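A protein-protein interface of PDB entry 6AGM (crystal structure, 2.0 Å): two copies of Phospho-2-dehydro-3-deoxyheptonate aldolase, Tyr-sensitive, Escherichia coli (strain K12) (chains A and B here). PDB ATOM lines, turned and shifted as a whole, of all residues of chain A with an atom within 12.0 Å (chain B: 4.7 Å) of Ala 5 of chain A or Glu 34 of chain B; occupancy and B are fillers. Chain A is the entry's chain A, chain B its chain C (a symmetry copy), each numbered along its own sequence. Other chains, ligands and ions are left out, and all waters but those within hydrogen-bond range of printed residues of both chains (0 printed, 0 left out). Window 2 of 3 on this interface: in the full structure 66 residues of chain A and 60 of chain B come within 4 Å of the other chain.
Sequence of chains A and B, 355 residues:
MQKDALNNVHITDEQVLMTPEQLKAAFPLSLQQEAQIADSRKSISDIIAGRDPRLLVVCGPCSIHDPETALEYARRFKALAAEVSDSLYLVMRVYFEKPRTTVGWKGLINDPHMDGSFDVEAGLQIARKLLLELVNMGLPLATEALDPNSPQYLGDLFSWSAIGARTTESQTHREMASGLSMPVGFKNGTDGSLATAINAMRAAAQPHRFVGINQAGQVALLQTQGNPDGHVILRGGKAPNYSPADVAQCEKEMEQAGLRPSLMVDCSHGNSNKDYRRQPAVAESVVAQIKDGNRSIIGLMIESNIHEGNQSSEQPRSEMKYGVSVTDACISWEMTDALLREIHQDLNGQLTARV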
ATOM      1  N   ASP A   4     -20.401 -14.775 -18.794  1.00  0.00           N
ATOM      2  CA  ASP A   4     -19.621 -14.296 -17.660  1.00  0.00           C
ATOM      3  C   ASP A   4     -19.612 -12.771 -17.609  1.00  0.00           C
ATOM      4  O   ASP A   4     -19.288 -12.108 -18.595  1.00  0.00           O
ATOM      5  CB  ASP A   4     -18.189 -14.830 -17.729  1.00  0.00           C
ATOM      6  CG  ASP A   4     -17.514 -14.873 -16.369  1.00  0.00           C
ATOM      7  OD1 ASP A   4     -17.699 -13.926 -15.575  1.00  0.00           O
ATOM      8  OD2 ASP A   4     -16.797 -15.856 -16.094  1.00  0.00           O
ATOM      9  N   ALA A   5     -19.965 -12.221 -16.451  1.00  0.00           N
ATOM     10  CA  ALA A   5     -20.014 -10.780 -16.254  1.00  0.00           C
ATOM     11  C   ALA A   5     -18.688 -10.196 -15.785  1.00  0.00           C
ATOM     12  O   ALA A   5     -18.594  -8.976 -15.608  1.00  0.00           O
ATOM     13  CB  ALA A   5     -21.115 -10.422 -15.250  1.00  0.00           C
ATOM     14  N   LEU A   6     -17.664 -11.026 -15.585  1.00  0.00           N
ATOM     15  CA  LEU A   6     -16.399 -10.542 -15.049  1.00  0.00           C
ATOM     16  C   LEU A   6     -15.221 -10.946 -15.927  1.00  0.00           C
ATOM     17  O   LEU A   6     -14.200 -10.251 -15.959  1.00  0.00           O
ATOM     18  CB  LEU A   6     -16.195 -11.063 -13.624  1.00  0.00           C
ATOM     19  CG  LEU A   6     -15.781 -10.032 -12.575  1.00  0.00           C
ATOM     20  CD1 LEU A   6     -16.638  -8.779 -12.680  1.00  0.00           C
ATOM     21  CD2 LEU A   6     -15.871 -10.629 -11.184  1.00  0.00           C
ATOM     22  N   ASN A   7     -15.352 -12.057 -16.647  1.00  0.00           N
ATOM     23  CA  ASN A   7     -14.251 -12.632 -17.409  1.00  0.00           C
ATOM     24  C   ASN A   7     -14.479 -12.438 -18.901  1.00  0.00           C
ATOM     25  O   ASN A   7     -15.563 -12.740 -19.415  1.00  0.00           O
ATOM     26  CB  ASN A   7     -14.087 -14.119 -17.089  1.00  0.00           C
ATOM     27  CG  ASN A   7     -13.322 -14.358 -15.801  1.00  0.00           C
ATOM     28  OD1 ASN A   7     -12.091 -14.327 -15.783  1.00  0.00           O
ATOM     29  ND2 ASN A   7     -14.048 -14.603 -14.714  1.00  0.00           N
ATOM     30  N   ASN A   8     -13.447 -11.939 -19.590  1.00  0.00           N
ATOM     31  CA  ASN A   8     -13.446 -11.796 -21.047  1.00  0.00           C
ATOM     32  C   ASN A   8     -14.633 -10.978 -21.542  1.00  0.00           C
ATOM     33  O   ASN A   8     -15.186 -11.252 -22.609  1.00  0.00           O
ATOM     34  CB  ASN A   8     -13.409 -13.163 -21.736  1.00  0.00           C
ATOM     35  CG  ASN A   8     -12.050 -13.831 -21.625  1.00  0.00           C
ATOM     36  OD1 ASN A   8     -11.245 -13.484 -20.760  1.00  0.00           O
ATOM     37  ND2 ASN A   8     -11.789 -14.798 -22.497  1.00  0.00           N
ATOM     38  N   VAL A   9     -15.032  -9.971 -20.763  1.00  0.00           N
ATOM     39  CA  VAL A   9     -16.131  -9.100 -21.166  1.00  0.00           C
ATOM     40  C   VAL A   9     -15.836  -8.456 -22.514  1.00  0.00           C
ATOM     41  O   VAL A   9     -16.711  -8.370 -23.385  1.00  0.00           O
ATOM     42  CB  VAL A   9     -16.390  -8.042 -20.079  1.00  0.00           C
ATOM     43  CG1 VAL A   9     -17.593  -7.187 -20.443  1.00  0.00           C
ATOM     44  CG2 VAL A   9     -16.584  -8.711 -18.727  1.00  0.00           C
ATOM     45  N   HIS A  10     -14.599  -8.002 -22.712  1.00  0.00           N
ATOM     46  CA  HIS A  10     -14.200  -7.319 -23.935  1.00  0.00           C
ATOM     47  C   HIS A  10     -13.379  -8.214 -24.855  1.00  0.00           C
ATOM     48  O   HIS A  10     -12.556  -7.722 -25.637  1.00  0.00           O
ATOM     49  CB  HIS A  10     -13.432  -6.044 -23.593  1.00  0.00           C
ATOM     50  CG  HIS A  10     -14.232  -5.064 -22.792  1.00  0.00           C
ATOM     51  ND1 HIS A  10     -15.567  -4.824 -23.036  1.00  0.00           N
ATOM     52  CD2 HIS A  10     -13.893  -4.278 -21.744  1.00  0.00           C
ATOM     53  CE1 HIS A  10     -16.013  -3.923 -22.179  1.00  0.00           C
ATOM     54  NE2 HIS A  10     -15.017  -3.577 -21.382  1.00  0.00           N
ATOM     55  N   ILE A  11     -13.583  -9.523 -24.768  1.00  0.00           N
ATOM     56  CA  ILE A  11     -12.941 -10.492 -25.644  1.00  0.00           C
ATOM     57  C   ILE A  11     -14.031 -11.214 -26.419  1.00  0.00           C
ATOM     58  O   ILE A  11     -14.979 -11.736 -25.823  1.00  0.00           O
ATOM     59  CB  ILE A  11     -12.073 -11.487 -24.853  1.00  0.00           C
ATOM     60  CG1 ILE A  11     -10.794 -10.793 -24.382  1.00  0.00           C
ATOM     61  CG2 ILE A  11     -11.758 -12.712 -25.699  1.00  0.00           C
ATOM     62  CD1 ILE A  11      -9.756 -11.735 -23.883  1.00  0.00           C
ATOM     63  N   LEU B  29     -14.582 -17.363  -7.085  1.00  0.00           N
ATOM     64  CA  LEU B  29     -15.376 -16.237  -6.629  1.00  0.00           C
ATOM     65  C   LEU B  29     -16.773 -16.707  -6.250  1.00  0.00           C
ATOM     66  O   LEU B  29     -17.316 -17.642  -6.843  1.00  0.00           O
ATOM     67  CB  LEU B  29     -15.475 -15.166  -7.716  1.00  0.00           C
ATOM     68  CG  LEU B  29     -14.329 -14.161  -7.832  1.00  0.00           C
ATOM     69  CD1 LEU B  29     -14.504 -13.303  -9.073  1.00  0.00           C
ATOM     70  CD2 LEU B  29     -14.269 -13.294  -6.595  1.00  0.00           C
ATOM     71  N   SER B  30     -17.346 -16.057  -5.246  1.00  0.00           N
ATOM     72  CA  SER B  30     -18.759 -16.228  -4.960  1.00  0.00           C
ATOM     73  C   SER B  30     -19.575 -15.249  -5.799  1.00  0.00           C
ATOM     74  O   SER B  30     -19.049 -14.294  -6.374  1.00  0.00           O
ATOM     75  CB  SER B  30     -19.039 -16.035  -3.468  1.00  0.00           C
ATOM     76  OG  SER B  30     -18.575 -14.777  -3.012  1.00  0.00           O
ATOM     77  N   LEU B  31     -20.884 -15.501  -5.871  1.00  0.00           N
ATOM     78  CA  LEU B  31     -21.767 -14.612  -6.619  1.00  0.00           C
ATOM     79  C   LEU B  31     -21.744 -13.203  -6.037  1.00  0.00           C
ATOM     80  O   LEU B  31     -21.781 -12.211  -6.779  1.00  0.00           O
ATOM     81  CB  LEU B  31     -23.191 -15.167  -6.622  1.00  0.00           C
ATOM     82  CG  LEU B  31     -23.490 -16.324  -7.583  1.00  0.00           C
ATOM     83  CD1 LEU B  31     -24.904 -16.850  -7.371  1.00  0.00           C
ATOM     84  CD2 LEU B  31     -23.274 -15.918  -9.035  1.00  0.00           C
ATOM     85  N   GLN B  32     -21.659 -13.096  -4.712  1.00  0.00           N
ATOM     86  CA  GLN B  32     -21.629 -11.781  -4.090  1.00  0.00           C
ATOM     87  C   GLN B  32     -20.349 -11.035  -4.452  1.00  0.00           C
ATOM     88  O   GLN B  32     -20.401  -9.858  -4.827  1.00  0.00           O
ATOM     89  CB  GLN B  32     -21.787 -11.933  -2.569  1.00  0.00           C
ATOM     90  CG  GLN B  32     -23.171 -12.394  -2.124  1.00  0.00           C
ATOM     91  CD  GLN B  32     -23.201 -13.874  -1.750  1.00  0.00           C
ATOM     92  OE1 GLN B  32     -22.977 -14.744  -2.595  1.00  0.00           O
ATOM     93  NE2 GLN B  32     -23.457 -14.160  -0.479  1.00  0.00           N
ATOM     94  N   GLN B  33     -19.202 -11.718  -4.397  1.00  0.00           N
ATOM     95  CA  GLN B  33     -17.938 -11.083  -4.759  1.00  0.00           C
ATOM     96  C   GLN B  33     -17.931 -10.657  -6.223  1.00  0.00           C
ATOM     97  O   GLN B  33     -17.474  -9.555  -6.563  1.00  0.00           O
ATOM     98  CB  GLN B  33     -16.784 -12.041  -4.479  1.00  0.00           C
ATOM     99  CG  GLN B  33     -16.511 -12.285  -3.012  1.00  0.00           C
ATOM    100  CD  GLN B  33     -15.606 -13.479  -2.793  1.00  0.00           C
ATOM    101  OE1 GLN B  33     -15.728 -14.497  -3.474  1.00  0.00           O
ATOM    102  NE2 GLN B  33     -14.687 -13.357  -1.847  1.00  0.00           N
ATOM    103  N   GLU B  34     -18.427 -11.525  -7.104  1.00  0.00           N
ATOM    104  CA  GLU B  34     -18.502 -11.204  -8.525  1.00  0.00           C
ATOM    105  C   GLU B  34     -19.361  -9.969  -8.769  1.00  0.00           C
ATOM    106  O   GLU B  34     -18.977  -9.073  -9.535  1.00  0.00           O
ATOM    107  CB  GLU B  34     -19.051 -12.410  -9.287  1.00  0.00           C
ATOM    108  CG  GLU B  34     -19.063 -12.283 -10.796  1.00  0.00           C
ATOM    109  CD  GLU B  34     -19.613 -13.532 -11.465  1.00  0.00           C
ATOM    110  OE1 GLU B  34     -19.826 -13.504 -12.696  1.00  0.00           O
ATOM    111  OE2 GLU B  34     -19.834 -14.540 -10.756  1.00  0.00           O
ATOM    112  N   ALA B  35     -20.528  -9.901  -8.121  1.00  0.00           N
ATOM    113  CA  ALA B  35     -21.388  -8.732  -8.276  1.00  0.00           C
ATOM    114  C   ALA B  35     -20.720  -7.476  -7.728  1.00  0.00           C
ATOM    115  O   ALA B  35     -20.822  -6.398  -8.326  1.00  0.00           O
ATOM    116  CB  ALA B  35     -22.730  -8.970  -7.586  1.00  0.00           C
ATOM    117  N   GLN B  36     -20.034  -7.594  -6.590  1.00  0.00           N
ATOM    118  CA  GLN B  36     -19.348  -6.441  -6.015  1.00  0.00           C
ATOM    119  C   GLN B  36     -18.266  -5.919  -6.957  1.00  0.00           C
ATOM    120  O   GLN B  36     -18.119  -4.702  -7.133  1.00  0.00           O
ATOM    121  CB  GLN B  36     -18.754  -6.813  -4.658  1.00  0.00           C
ATOM    122  CG  GLN B  36     -17.882  -5.735  -4.042  1.00  0.00           C
ATOM    123  CD  GLN B  36     -16.873  -6.300  -3.063  1.00  0.00           C
ATOM    124  OE1 GLN B  36     -15.662  -6.169  -3.257  1.00  0.00           O
ATOM    125  NE2 GLN B  36     -17.365  -6.930  -2.001  1.00  0.00           N
ATOM    126  N   ILE B  37     -17.512  -6.826  -7.580  1.00  0.00           N
ATOM    127  CA  ILE B  37     -16.457  -6.410  -8.500  1.00  0.00           C
ATOM    128  C   ILE B  37     -17.050  -5.761  -9.746  1.00  0.00           C
ATOM    129  O   ILE B  37     -16.549  -4.733 -10.222  1.00  0.00           O
ATOM    130  CB  ILE B  37     -15.553  -7.605  -8.855  1.00  0.00           C
ATOM    131  CG1 ILE B  37     -14.808  -8.097  -7.610  1.00  0.00           C
ATOM    132  CG2 ILE B  37     -14.568  -7.221  -9.953  1.00  0.00           C
ATOM    133  CD1 ILE B  37     -14.108  -9.429  -7.796  1.00  0.00           C
ATOM    134  N   ALA B  38     -18.117  -6.346 -10.300  1.00  0.00           N
ATOM    135  CA  ALA B  38     -18.770  -5.728 -11.452  1.00  0.00           C
ATOM    136  C   ALA B  38     -19.288  -4.336 -11.105  1.00  0.00           C
ATOM    137  O   ALA B  38     -19.176  -3.401 -11.910  1.00  0.00           O
ATOM    138  CB  ALA B  38     -19.908  -6.616 -11.953  1.00  0.00           C
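The backbone NH of Leu 6 of chain A sits at hydrogen-bond distance from the side-chain carboxylate of Asp 4 of chain A (2.9 Å). N of Asn 7 of chain A sits at hydrogen-bond distance from OD1 of Asp 4 of chain A.
Of the 10 printed residues of chain B, 4 touch a printed residue of chain A. Printed residues of chain B that touch a printed residue of chain A: Leu 29, Glu 34, Ile 37 and Ala 38. Along chain B the printed residues that touch a printed residue of chain A span positions 29 to 38. Printed residues of chain A that touch a printed residue of chain B: Asp 4, Ala 5 and Leu 6. Hydrophobic or aromatic side chains of chain A within 4 Å of the printed part of chain B: Leu 6. Among the printed residues, 6 pairs touch across the chains. Among the printed residues, no Asp or Glu carboxylate lies within 4 Å of a Lys or Arg side-chain nitrogen of the other chain.
Ala 5 of chain A touches one residue of chain B. Glu 34 of chain B touches three residues of chain A. Leu 29 of chain B touches just one residue of chain A: Leu 6. No residue of chain A comes within 4 Å of Ser 30 of chain B. No residue of chain A comes within 4 Å of Leu 31 of chain B. No residue of chain A comes within 4 Å of Gln 33 of chain B. No residue of chain A comes within 4 Å of Gln 36 of chain B. Ile 37 of chain B touches one residue of chain A. Of chain A, only Leu 6 (3.7 Å) comes within 4 Å of Ala 38 of chain B. Of the printed residues of chain B, Asp 4 of chain A touches Glu 34. Printed residues of chain B within 4 Å of Leu 6 of chain A: Leu 29, Glu 34, Ile 37 and Ala 38. The nearest residue of chain B that does not touch Ala 5 of chain A is Ala 38 of chain B (4.5 Å). The nearest residue of chain A that does not touch Glu 34 of chain B is Asn 7 of chain A (6.1 Å).
No position is printed for both chains.
Glu 34 of chain B touches Asp 4 of chain A (OE1 to OD1, 3.6 Å). Ala 5 of chain A touches Glu 34 of chain B (N to OE1, 3.97 Å). Leu 29 of chain B touches Leu 6 of chain A. Glu 34 of chain B touches Leu 6 of chain A (CG to CD2, 3.6 Å). Leu 6 of chain A touches Ile 37 of chain B. Leu 6 of chain A touches Ala 38 of chain B (CD1 to N, 3.7 Å).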
